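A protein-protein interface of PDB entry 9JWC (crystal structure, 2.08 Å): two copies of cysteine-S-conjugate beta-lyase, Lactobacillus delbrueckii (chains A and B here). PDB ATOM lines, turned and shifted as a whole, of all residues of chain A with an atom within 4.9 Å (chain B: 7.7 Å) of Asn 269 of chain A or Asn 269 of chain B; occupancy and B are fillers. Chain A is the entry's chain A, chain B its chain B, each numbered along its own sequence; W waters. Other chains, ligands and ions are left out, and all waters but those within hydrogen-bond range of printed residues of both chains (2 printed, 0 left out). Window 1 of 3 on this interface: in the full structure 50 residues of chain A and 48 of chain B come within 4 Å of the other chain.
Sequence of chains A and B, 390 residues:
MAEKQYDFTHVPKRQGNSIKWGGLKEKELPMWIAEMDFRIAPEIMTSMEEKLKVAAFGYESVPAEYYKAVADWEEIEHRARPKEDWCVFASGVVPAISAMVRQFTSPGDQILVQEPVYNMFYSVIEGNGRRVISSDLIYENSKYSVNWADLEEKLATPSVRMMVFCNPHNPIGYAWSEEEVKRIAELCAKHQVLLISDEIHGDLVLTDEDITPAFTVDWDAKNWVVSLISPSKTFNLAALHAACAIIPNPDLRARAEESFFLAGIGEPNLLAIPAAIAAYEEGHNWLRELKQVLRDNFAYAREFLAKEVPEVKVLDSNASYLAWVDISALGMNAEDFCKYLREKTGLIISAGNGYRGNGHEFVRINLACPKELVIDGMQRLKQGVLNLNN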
ATOM      1  N   GLU A  60     -35.330 -27.233  22.814  1.00  0.00           N
ATOM      2  CA  GLU A  60     -35.876 -26.190  23.657  1.00  0.00           C
ATOM      3  C   GLU A  60     -37.144 -25.609  23.071  1.00  0.00           C
ATOM      4  O   GLU A  60     -37.254 -25.439  21.854  1.00  0.00           O
ATOM      5  CB  GLU A  60     -34.859 -25.107  23.857  1.00  0.00           C
ATOM      6  CG  GLU A  60     -33.892 -25.569  24.877  1.00  0.00           C
ATOM      7  CD  GLU A  60     -32.953 -24.512  25.258  1.00  0.00           C
ATOM      8  OE1 GLU A  60     -31.788 -24.865  25.497  1.00  0.00           O
ATOM      9  OE2 GLU A  60     -33.399 -23.345  25.325  1.00  0.00           O
ATOM     10  N   ALA A 239     -23.946 -13.084  17.624  1.00  0.00           N
ATOM     11  CA  ALA A 239     -23.838 -14.527  17.475  1.00  0.00           C
ATOM     12  C   ALA A 239     -24.750 -15.285  18.436  1.00  0.00           C
ATOM     13  O   ALA A 239     -24.735 -16.513  18.438  1.00  0.00           O
ATOM     14  CB  ALA A 239     -22.383 -14.973  17.661  1.00  0.00           C
ATOM     15  N   LEU A 240     -25.574 -14.590  19.222  1.00  0.00           N
ATOM     16  CA  LEU A 240     -26.530 -15.292  20.077  1.00  0.00           C
ATOM     17  C   LEU A 240     -27.652 -15.919  19.265  1.00  0.00           C
ATOM     18  O   LEU A 240     -28.156 -16.993  19.626  1.00  0.00           O
ATOM     19  CB  LEU A 240     -27.125 -14.337  21.105  1.00  0.00           C
ATOM     20  CG  LEU A 240     -28.182 -14.980  22.007  1.00  0.00           C
ATOM     21  CD1 LEU A 240     -27.566 -16.169  22.765  1.00  0.00           C
ATOM     22  CD2 LEU A 240     -28.795 -13.958  22.965  1.00  0.00           C
ATOM     23  N   HIS A 241     -28.047 -15.265  18.176  1.00  0.00           N
ATOM     24  CA  HIS A 241     -29.142 -15.720  17.315  1.00  0.00           C
ATOM     25  C   HIS A 241     -30.451 -15.829  18.090  1.00  0.00           C
ATOM     26  O   HIS A 241     -31.143 -16.853  18.055  1.00  0.00           O
ATOM     27  CB  HIS A 241     -28.792 -17.040  16.631  1.00  0.00           C
ATOM     28  CG  HIS A 241     -27.621 -16.939  15.706  1.00  0.00           C
ATOM     29  ND1 HIS A 241     -27.103 -18.028  15.042  1.00  0.00           N
ATOM     30  CD2 HIS A 241     -26.883 -15.873  15.310  1.00  0.00           C
ATOM     31  CE1 HIS A 241     -26.088 -17.643  14.291  1.00  0.00           C
ATOM     32  NE2 HIS A 241     -25.924 -16.341  14.444  1.00  0.00           N
ATOM     33  N   GLU A 267     -36.384 -22.087  15.894  1.00  0.00           N
ATOM     34  CA  GLU A 267     -36.037 -22.858  17.099  1.00  0.00           C
ATOM     35  C   GLU A 267     -34.845 -22.245  17.861  1.00  0.00           C
ATOM     36  O   GLU A 267     -33.831 -22.013  17.253  1.00  0.00           O
ATOM     37  CB  GLU A 267     -35.753 -24.303  16.728  1.00  0.00           C
ATOM     38  CG  GLU A 267     -35.145 -25.102  17.864  1.00  0.00           C
ATOM     39  CD  GLU A 267     -34.844 -26.559  17.572  1.00  0.00           C
ATOM     40  OE1 GLU A 267     -35.755 -27.262  17.105  1.00  0.00           O
ATOM     41  OE2 GLU A 267     -33.707 -26.981  17.830  1.00  0.00           O
ATOM     42  N   PRO A 268     -34.938 -22.004  19.196  1.00  0.00           N
ATOM     43  CA  PRO A 268     -33.800 -21.390  19.880  1.00  0.00           C
ATOM     44  C   PRO A 268     -32.661 -22.374  20.041  1.00  0.00           C
ATOM     45  O   PRO A 268     -32.867 -23.558  20.335  1.00  0.00           O
ATOM     46  CB  PRO A 268     -34.367 -20.965  21.239  1.00  0.00           C
ATOM     47  CG  PRO A 268     -35.581 -21.810  21.448  1.00  0.00           C
ATOM     48  CD  PRO A 268     -36.109 -22.177  20.074  1.00  0.00           C
ATOM     49  N   ASN A 269     -31.445 -21.854  19.874  1.00  0.00           N
ATOM     50  CA  ASN A 269     -30.258 -22.613  20.222  1.00  0.00           C
ATOM     51  C   ASN A 269     -30.109 -22.652  21.744  1.00  0.00           C
ATOM     52  O   ASN A 269     -30.936 -22.130  22.493  1.00  0.00           O
ATOM     53  CB  ASN A 269     -29.019 -22.036  19.524  1.00  0.00           C
ATOM     54  CG  ASN A 269     -28.676 -20.615  19.972  1.00  0.00           C
ATOM     55  OD1 ASN A 269     -28.677 -20.308  21.156  1.00  0.00           O
ATOM     56  ND2 ASN A 269     -28.358 -19.752  19.011  1.00  0.00           N
ATOM     57  N   LEU A 270     -29.029 -23.279  22.210  1.00  0.00           N
ATOM     58  CA  LEU A 270     -28.863 -23.596  23.626  1.00  0.00           C
ATOM     59  C   LEU A 270     -28.708 -22.375  24.529  1.00  0.00           C
ATOM     60  O   LEU A 270     -28.840 -22.512  25.753  1.00  0.00           O
ATOM     61  CB  LEU A 270     -27.657 -24.520  23.811  1.00  0.00           C
ATOM     62  CG  LEU A 270     -26.242 -23.943  23.701  1.00  0.00           C
ATOM     63  CD1 LEU A 270     -25.237 -25.089  23.761  1.00  0.00           C
ATOM     64  CD2 LEU A 270     -26.024 -23.140  22.415  1.00  0.00           C
ATOM     65  N   LEU A 271     -28.441 -21.193  23.983  1.00  0.00           N
ATOM     66  CA  LEU A 271     -28.305 -20.002  24.808  1.00  0.00           C
ATOM     67  C   LEU A 271     -29.344 -18.925  24.521  1.00  0.00           C
ATOM     68  O   LEU A 271     -29.486 -18.002  25.330  1.00  0.00           O
ATOM     69  CB  LEU A 271     -26.904 -19.393  24.635  1.00  0.00           C
ATOM     70  CG  LEU A 271     -25.740 -20.167  25.257  1.00  0.00           C
ATOM     71  CD1 LEU A 271     -24.433 -19.393  25.084  1.00  0.00           C
ATOM     72  CD2 LEU A 271     -26.013 -20.403  26.723  1.00  0.00           C
ATOM     73  N   ALA A 272     -30.082 -19.022  23.414  1.00  0.00           N
ATOM     74  CA  ALA A 272     -30.909 -17.906  22.963  1.00  0.00           C
ATOM     75  C   ALA A 272     -31.945 -17.503  24.008  1.00  0.00           C
ATOM     76  O   ALA A 272     -32.147 -16.308  24.262  1.00  0.00           O
ATOM     77  CB  ALA A 272     -31.591 -18.270  21.637  1.00  0.00           C
ATOM     78  N   ILE A 273     -32.597 -18.471  24.641  1.00  0.00           N
ATOM     79  CA  ILE A 273     -33.701 -18.121  25.536  1.00  0.00           C
ATOM     80  C   ILE A 273     -33.169 -17.525  26.835  1.00  0.00           C
ATOM     81  O   ILE A 273     -33.552 -16.395  27.174  1.00  0.00           O
ATOM     82  CB  ILE A 273     -34.625 -19.320  25.800  1.00  0.00           C
ATOM     83  CG1 ILE A 273     -35.295 -19.757  24.500  1.00  0.00           C
ATOM     84  CG2 ILE A 273     -35.691 -18.934  26.836  1.00  0.00           C
ATOM     85  CD1 ILE A 273     -36.033 -18.625  23.828  1.00  0.00           C
ATOM     86  N   ASN B  17     -37.738 -24.826  29.973  1.00  0.00           N
ATOM     87  CA  ASN B  17     -38.212 -24.836  28.592  1.00  0.00           C
ATOM     88  C   ASN B  17     -37.692 -26.032  27.799  1.00  0.00           C
ATOM     89  O   ASN B  17     -37.522 -25.942  26.577  1.00  0.00           O
ATOM     90  CB  ASN B  17     -37.840 -23.530  27.887  1.00  0.00           C
ATOM     91  CG  ASN B  17     -36.358 -23.405  27.638  1.00  0.00           C
ATOM     92  OD1 ASN B  17     -35.546 -23.845  28.440  1.00  0.00           O
ATOM     93  ND2 ASN B  17     -35.998 -22.814  26.507  1.00  0.00           N
ATOM     94  N   LYS B  51     -15.075 -20.554  25.423  1.00  0.00           N
ATOM     95  CA  LYS B  51     -15.588 -19.573  24.468  1.00  0.00           C
ATOM     96  C   LYS B  51     -16.340 -18.455  25.179  1.00  0.00           C
ATOM     97  O   LYS B  51     -16.230 -17.285  24.796  1.00  0.00           O
ATOM     98  CB  LYS B  51     -16.476 -20.283  23.429  1.00  0.00           C
ATOM     99  CG  LYS B  51     -17.127 -19.342  22.420  1.00  0.00           C
ATOM    100  CD  LYS B  51     -16.110 -18.473  21.704  1.00  0.00           C
ATOM    101  CE  LYS B  51     -16.782 -17.628  20.613  1.00  0.00           C
ATOM    102  NZ  LYS B  51     -17.246 -18.471  19.451  1.00  0.00           N
ATOM    103  N   PHE B  57     -19.881 -11.362  21.790  1.00  0.00           N
ATOM    104  CA  PHE B  57     -20.318 -12.399  20.862  1.00  0.00           C
ATOM    105  C   PHE B  57     -20.805 -11.762  19.564  1.00  0.00           C
ATOM    106  O   PHE B  57     -21.985 -11.791  19.215  1.00  0.00           O
ATOM    107  CB  PHE B  57     -21.346 -13.281  21.546  1.00  0.00           C
ATOM    108  CG  PHE B  57     -20.808 -13.865  22.811  1.00  0.00           C
ATOM    109  CD1 PHE B  57     -19.751 -14.759  22.760  1.00  0.00           C
ATOM    110  CD2 PHE B  57     -21.266 -13.442  24.046  1.00  0.00           C
ATOM    111  CE1 PHE B  57     -19.211 -15.271  23.933  1.00  0.00           C
ATOM    112  CE2 PHE B  57     -20.726 -13.948  25.225  1.00  0.00           C
ATOM    113  CZ  PHE B  57     -19.708 -14.853  25.171  1.00  0.00           C
ATOM    114  N   GLY B  58     -19.846 -11.198  18.836  1.00  0.00           N
ATOM    115  CA  GLY B  58     -20.089 -10.639  17.528  1.00  0.00           C
ATOM    116  C   GLY B  58     -20.027 -11.710  16.460  1.00  0.00           C
ATOM    117  O   GLY B  58     -20.097 -12.911  16.731  1.00  0.00           O
ATOM    118  N   GLU B  60     -19.091 -14.297  13.583  1.00  0.00           N
ATOM    119  CA  GLU B  60     -18.076 -15.332  13.482  1.00  0.00           C
ATOM    120  C   GLU B  60     -17.973 -15.854  12.062  1.00  0.00           C
ATOM    121  O   GLU B  60     -18.986 -16.045  11.381  1.00  0.00           O
ATOM    122  CB  GLU B  60     -18.398 -16.483  14.405  1.00  0.00           C
ATOM    123  CG  GLU B  60     -18.500 -16.024  15.813  1.00  0.00           C
ATOM    124  CD  GLU B  60     -18.278 -17.134  16.774  1.00  0.00           C
ATOM    125  OE1 GLU B  60     -18.534 -16.889  17.966  1.00  0.00           O
ATOM    126  OE2 GLU B  60     -17.862 -18.238  16.334  1.00  0.00           O
ATOM    127  N   SER B  61     -16.745 -16.085  11.629  1.00  0.00           N
ATOM    128  CA  SER B  61     -16.516 -16.815  10.398  1.00  0.00           C
ATOM    129  C   SER B  61     -16.451 -18.302  10.727  1.00  0.00           C
ATOM    130  O   SER B  61     -16.449 -18.704  11.892  1.00  0.00           O
ATOM    131  CB  SER B  61     -15.224 -16.344   9.742  1.00  0.00           C
ATOM    132  OG  SER B  61     -14.137 -16.621  10.601  1.00  0.00           O
ATOM    133  N   PHE B  89     -20.421 -25.222   6.547  1.00  0.00           N
ATOM    134  CA  PHE B  89     -21.188 -25.127   7.777  1.00  0.00           C
ATOM    135  C   PHE B  89     -22.649 -24.841   7.475  1.00  0.00           C
ATOM    136  O   PHE B  89     -22.971 -24.042   6.596  1.00  0.00           O
ATOM    137  CB  PHE B  89     -20.620 -24.018   8.667  1.00  0.00           C
ATOM    138  CG  PHE B  89     -21.398 -23.813   9.933  1.00  0.00           C
ATOM    139  CD1 PHE B  89     -22.483 -22.947   9.971  1.00  0.00           C
ATOM    140  CD2 PHE B  89     -21.056 -24.509  11.083  1.00  0.00           C
ATOM    141  CE1 PHE B  89     -23.218 -22.781  11.139  1.00  0.00           C
ATOM    142  CE2 PHE B  89     -21.785 -24.352  12.246  1.00  0.00           C
ATOM    143  CZ  PHE B  89     -22.866 -23.487  12.278  1.00  0.00           C
ATOM    144  N   SER B  91     -26.393 -24.427  10.058  1.00  0.00           N
ATOM    145  CA  SER B  91     -26.805 -24.422  11.455  1.00  0.00           C
ATOM    146  C   SER B  91     -27.591 -25.662  11.854  1.00  0.00           C
ATOM    147  O   SER B  91     -27.830 -25.878  13.045  1.00  0.00           O
ATOM    148  CB  SER B  91     -27.629 -23.172  11.740  1.00  0.00           C
ATOM    149  OG  SER B  91     -26.748 -22.080  11.934  1.00  0.00           O
ATOM    150  N   ALA B 238     -28.515 -31.151  20.360  1.00  0.00           N
ATOM    151  CA  ALA B 238     -29.561 -30.694  19.439  1.00  0.00           C
ATOM    152  C   ALA B 238     -29.616 -29.172  19.347  1.00  0.00           C
ATOM    153  O   ALA B 238     -29.694 -28.604  18.249  1.00  0.00           O
ATOM    154  CB  ALA B 238     -30.929 -31.239  19.869  1.00  0.00           C
ATOM    155  N   ALA B 239     -29.586 -28.491  20.493  1.00  0.00           N
ATOM    156  CA  ALA B 239     -29.694 -27.043  20.497  1.00  0.00           C
ATOM    157  C   ALA B 239     -28.371 -26.340  20.215  1.00  0.00           C
ATOM    158  O   ALA B 239     -28.333 -25.108  20.257  1.00  0.00           O
ATOM    159  CB  ALA B 239     -30.260 -26.550  21.839  1.00  0.00           C
ATOM    160  N   LEU B 240     -27.294 -27.062  19.903  1.00  0.00           N
ATOM    161  CA  LEU B 240     -26.064 -26.361  19.548  1.00  0.00           C
ATOM    162  C   LEU B 240     -26.194 -25.706  18.180  1.00  0.00           C
ATOM    163  O   LEU B 240     -25.644 -24.622  17.945  1.00  0.00           O
ATOM    164  CB  LEU B 240     -24.865 -27.311  19.563  1.00  0.00           C
ATOM    165  CG  LEU B 240     -23.526 -26.669  19.133  1.00  0.00           C
ATOM    166  CD1 LEU B 240     -23.090 -25.590  20.135  1.00  0.00           C
ATOM    167  CD2 LEU B 240     -22.432 -27.726  18.986  1.00  0.00           C
ATOM    168  N   HIS B 241     -26.903 -26.361  17.264  1.00  0.00           N
ATOM    169  CA  HIS B 241     -27.138 -25.835  15.924  1.00  0.00           C
ATOM    170  C   HIS B 241     -25.816 -25.708  15.168  1.00  0.00           C
ATOM    171  O   HIS B 241     -25.478 -24.658  14.612  1.00  0.00           O
ATOM    172  CB  HIS B 241     -27.899 -24.500  15.968  1.00  0.00           C
ATOM    173  CG  HIS B 241     -29.301 -24.614  16.502  1.00  0.00           C
ATOM    174  ND1 HIS B 241     -30.151 -23.531  16.595  1.00  0.00           N
ATOM    175  CD2 HIS B 241     -30.002 -25.682  16.953  1.00  0.00           C
ATOM    176  CE1 HIS B 241     -31.310 -23.923  17.094  1.00  0.00           C
ATOM    177  NE2 HIS B 241     -31.244 -25.224  17.325  1.00  0.00           N
ATOM    178  N   ALA B 242     -25.053 -26.797  15.177  1.00  0.00           N
ATOM    179  CA  ALA B 242     -23.864 -26.934  14.349  1.00  0.00           C
ATOM    180  C   ALA B 242     -24.049 -28.149  13.450  1.00  0.00           C
ATOM    181  O   ALA B 242     -24.416 -29.232  13.922  1.00  0.00           O
ATOM    182  CB  ALA B 242     -22.604 -27.080  15.194  1.00  0.00           C
ATOM    183  N   GLY B 266     -26.453 -20.140   7.633  1.00  0.00           N
ATOM    184  CA  GLY B 266     -25.082 -20.308   7.180  1.00  0.00           C
ATOM    185  C   GLY B 266     -24.044 -19.793   8.155  1.00  0.00           C
ATOM    186  O   GLY B 266     -22.841 -20.011   7.968  1.00  0.00           O
ATOM    187  N   GLU B 267     -24.523 -19.054   9.155  1.00  0.00           N
ATOM    188  CA  GLU B 267     -23.628 -18.375  10.121  1.00  0.00           C
ATOM    189  C   GLU B 267     -23.602 -19.082  11.496  1.00  0.00           C
ATOM    190  O   GLU B 267     -24.643 -19.276  12.063  1.00  0.00           O
ATOM    191  CB  GLU B 267     -24.040 -16.910  10.251  1.00  0.00           C
ATOM    192  CG  GLU B 267     -23.318 -16.105  11.310  1.00  0.00           C
ATOM    193  CD  GLU B 267     -23.941 -14.746  11.603  1.00  0.00           C
ATOM    194  OE1 GLU B 267     -24.106 -13.962  10.653  1.00  0.00           O
ATOM    195  OE2 GLU B 267     -24.267 -14.478  12.780  1.00  0.00           O
ATOM    196  N   PRO B 268     -22.425 -19.445  12.059  1.00  0.00           N
ATOM    197  CA  PRO B 268     -22.426 -20.104  13.368  1.00  0.00           C
ATOM    198  C   PRO B 268     -22.880 -19.170  14.470  1.00  0.00           C
ATOM    199  O   PRO B 268     -22.536 -17.983  14.488  1.00  0.00           O
ATOM    200  CB  PRO B 268     -20.959 -20.509  13.567  1.00  0.00           C
ATOM    201  CG  PRO B 268     -20.199 -19.582  12.687  1.00  0.00           C
ATOM    202  CD  PRO B 268     -21.071 -19.308  11.507  1.00  0.00           C
ATOM    203  N   ASN B 269     -23.614 -19.732  15.427  1.00  0.00           N
ATOM    204  CA  ASN B 269     -23.860 -19.010  16.661  1.00  0.00           C
ATOM    205  C   ASN B 269     -22.605 -19.055  17.534  1.00  0.00           C
ATOM    206  O   ASN B 269     -21.572 -19.611  17.162  1.00  0.00           O
ATOM    207  CB  ASN B 269     -25.095 -19.565  17.378  1.00  0.00           C
ATOM    208  CG  ASN B 269     -24.898 -20.983  17.918  1.00  0.00           C
ATOM    209  OD1 ASN B 269     -23.911 -21.290  18.602  1.00  0.00           O
ATOM    210  ND2 ASN B 269     -25.874 -21.850  17.646  1.00  0.00           N
ATOM    211  N   LEU B 270     -22.717 -18.492  18.734  1.00  0.00           N
ATOM    212  CA  LEU B 270     -21.551 -18.189  19.557  1.00  0.00           C
ATOM    213  C   LEU B 270     -20.841 -19.425  20.086  1.00  0.00           C
ATOM    214  O   LEU B 270     -19.685 -19.320  20.504  1.00  0.00           O
ATOM    215  CB  LEU B 270     -21.964 -17.274  20.715  1.00  0.00           C
ATOM    216  CG  LEU B 270     -22.889 -17.784  21.835  1.00  0.00           C
ATOM    217  CD1 LEU B 270     -23.192 -16.651  22.801  1.00  0.00           C
ATOM    218  CD2 LEU B 270     -24.210 -18.396  21.346  1.00  0.00           C
ATOM    219  N   LEU B 271     -21.483 -20.593  20.073  1.00  0.00           N
ATOM    220  CA  LEU B 271     -20.825 -21.797  20.575  1.00  0.00           C
ATOM    221  C   LEU B 271     -20.595 -22.857  19.508  1.00  0.00           C
ATOM    222  O   LEU B 271     -19.831 -23.798  19.749  1.00  0.00           O
ATOM    223  CB  LEU B 271     -21.645 -22.406  21.715  1.00  0.00           C
ATOM    224  CG  LEU B 271     -21.694 -21.550  22.977  1.00  0.00           C
ATOM    225  CD1 LEU B 271     -22.540 -22.272  24.027  1.00  0.00           C
ATOM    226  CD2 LEU B 271     -20.284 -21.267  23.488  1.00  0.00           C
ATOM    227  N   ALA B 272     -21.209 -22.713  18.333  1.00  0.00           N
ATOM    228  CA  ALA B 272     -21.239 -23.800  17.362  1.00  0.00           C
ATOM    229  C   ALA B 272     -19.836 -24.241  16.948  1.00  0.00           C
ATOM    230  O   ALA B 272     -19.567 -25.444  16.824  1.00  0.00           O
ATOM    231  CB  ALA B 272     -22.056 -23.363  16.140  1.00  0.00           C
ATOM    232  N   ILE B 273     -18.933 -23.291  16.726  1.00  0.00           N
ATOM    233  CA  ILE B 273     -17.611 -23.596  16.185  1.00  0.00           C
ATOM    234  C   ILE B 273     -16.755 -24.275  17.251  1.00  0.00           C
ATOM    235  O   ILE B 273     -16.306 -25.409  17.028  1.00  0.00           O
ATOM    236  CB  ILE B 273     -16.922 -22.342  15.618  1.00  0.00           C
ATOM    237  CG1 ILE B 273     -17.675 -21.805  14.394  1.00  0.00           C
ATOM    238  CG2 ILE B 273     -15.457 -22.649  15.275  1.00  0.00           C
ATOM    239  CD1 ILE B 273     -18.065 -22.884  13.367  1.00  0.00           C
ATOM    240  N   PRO B 274     -16.492 -23.662  18.416  1.00  0.00           N
ATOM    241  CA  PRO B 274     -15.611 -24.354  19.380  1.00  0.00           C
ATOM    242  C   PRO B 274     -16.203 -25.653  19.904  1.00  0.00           C
ATOM    243  O   PRO B 274     -15.469 -26.635  20.077  1.00  0.00           O
ATOM    244  CB  PRO B 274     -15.416 -23.315  20.492  1.00  0.00           C
ATOM    245  CG  PRO B 274     -16.639 -22.450  20.415  1.00  0.00           C
ATOM    246  CD  PRO B 274     -16.947 -22.357  18.942  1.00  0.00           C
ATOM    247  N   ALA B 275     -17.521 -25.700  20.126  1.00  0.00           N
ATOM    248  CA  ALA B 275     -18.121 -26.913  20.666  1.00  0.00           C
ATOM    249  C   ALA B 275     -18.065 -28.056  19.659  1.00  0.00           C
ATOM    250  O   ALA B 275     -17.773 -29.197  20.033  1.00  0.00           O
ATOM    251  CB  ALA B 275     -19.562 -26.637  21.109  1.00  0.00           C
HETATM  252  O   HOH W   1     -32.364 -28.735  16.430  1.00  0.00           O
HETATM  253  O   HOH W   2     -28.088 -20.878  15.874  1.00  0.00           O
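Of the 23 printed residues of chain B, 10 touch a printed residue of chain A.
Printed residues of chain B that touch a printed residue of chain A: Asn 17, Phe 57, Gly 58, Ala 239, His 241, Glu 267, Pro 268, Asn 269, Leu 270 and Leu 271.
Hydrophobic or aromatic side chains of chain B that line the printed part of chain A: Ala 239, His 241, Leu 270 and Leu 271.
Along chain B the printed residues that touch a printed residue of chain A span positions 17 to 271.
Of the 11 printed residues of chain A, 9 touch a printed residue of chain B.
Hydrophobic or aromatic side chains of chain A that line the printed part of chain B: Ala 239, His 241, Leu 270, Leu 271 and Ile 273.
Among the printed residues, no Asp or Glu carboxylate lies within 4 Å of a Lys or Arg side-chain nitrogen of the other chain.
ND2 of Asn 269 of chain A lies within hydrogen-bond range of O of Leu 240 of chain A (2.8 Å).
OD1 of Asn 269 of chain A lies within hydrogen-bond range of N of Leu 271 of chain A (3.0 Å).
O of Leu 270 of chain B lies within hydrogen-bond range of NZ of Lys 51 of chain B (2.8 Å).
O of Leu 240 of chain B lies within hydrogen-bond range of ND2 of Asn 269 of chain B (2.8 Å).
The backbone NH (N) of Leu 271 of chain B sits at hydrogen-bond distance from the side-chain amide oxygen (OD1) of Asn 269 of chain B, 2.9 Å away.
The side-chain amide oxygen (OD1) of Asn 269 of chain B is in hydrogen-bond range of the backbone NH (N) of Ala 272 of chain B (3.1 Å).
Of chain B, only Ala 239 (3.2 Å), His 241 (3.5 Å) and Asn 269 (3.5 Å) come within 4 Å of Asn 269 of chain A.
Printed residues of chain B within 4 Å of His 241 of chain A: Glu 267, Pro 268 and Asn 269.
Of the printed residues of chain A, Pro 268 of chain B touches His 241.
Printed residues of chain A within 4 Å of Ala 239 of chain B: Asn 269 and Leu 270.
Glu 60 of chain B touches none of the printed residues of chain A.
The nearest residue of chain A that does not touch Asn 269 of chain B is Leu 240 of chain A (4.6 Å).
Water W1 bridges the side-chain carboxylate of Glu 267 of chain A (2.6 Å) and the backbone carbonyl oxygen of Ala 238 of chain B (3.2 Å).
Water W2 lies within hydrogen-bond range of the side-chain amide nitrogen of Asn 269 of chain B, a ring nitrogen (ND1) of His 241 of chain A, the side-chain amide nitrogen of Asn 269 of chain A and a ring nitrogen (ND1) of His 241 of chain B.
Among the printed residues, merely in contact across the chains: Asn 269 of chain A with Ala 239 of chain B, Ala 239 of chain A with Asn 269 of chain B, Ala 239 of chain A with Gly 58 of chain B, His 241 of chain A with Asn 269 of chain B, Asn 269 of chain A with His 241 of chain B, Asn 269 of chain A with Asn 269 of chain B, His 241 of chain A with Pro 268 of chain B, Pro 268 of chain A with His 241 of chain B, Leu 271 of chain A with Leu 271 of chain B, Ile 273 of chain A with Asn 17 of chain B, Leu 271 of chain A with Leu 270 of chain B and Leu 270 of chain A with Leu 271 of chain B.
Ala 239 of chain A touches Asn 269 of chain B, and with the chains exchanged Asn 269 of chain A touches Ala 239 of chain B.
Ala 239 of chain A touches Leu 270 of chain B, and with the chains exchanged Leu 270 of chain A touches Ala 239 of chain B.
Asn 269 of chain B touches its own counterpart, Asn 269 of chain A.
Leu 270 of chain A touches Leu 271 of chain B, and with the chains exchanged Leu 271 of chain A touches Leu 270 of chain B.
Positions printed for both chains: 60, 239, 240, 241, 267, 268, 269, 270, 271, 272 and 273.
Of the 18 pairs that touch across the chains among the printed residues, 14 have their exchanged pair printed and touching as well.
The side-chain amide nitrogen of Asn 17 of chain B lies within hydrogen-bond range of the side-chain carboxylate of Glu 60 of chain A, at 2.9 Å.
The backbone carbonyl oxygen of Phe 57 of chain B is in hydrogen-bond range of the backbone NH of Ala 239 of chain A (2.8 Å).
The backbone carbonyl oxygen (O) of Ala 239 of chain A lies within hydrogen-bond range of the backbone NH (N) of Leu 270 of chain B, at 2.8 Å.
The side-chain carboxylate (OE2) of Glu 267 of chain B sits at hydrogen-bond distance from a ring nitrogen (NE2) of His 241 of chain A.
OE2 of Glu 267 of chain A sits at hydrogen-bond distance from NE2 of His 241 of chain B.
The backbone NH (N) of Leu 270 of chain A sits at hydrogen-bond distance from the backbone carbonyl oxygen (O) of Ala 239 of chain B (2.8 Å).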
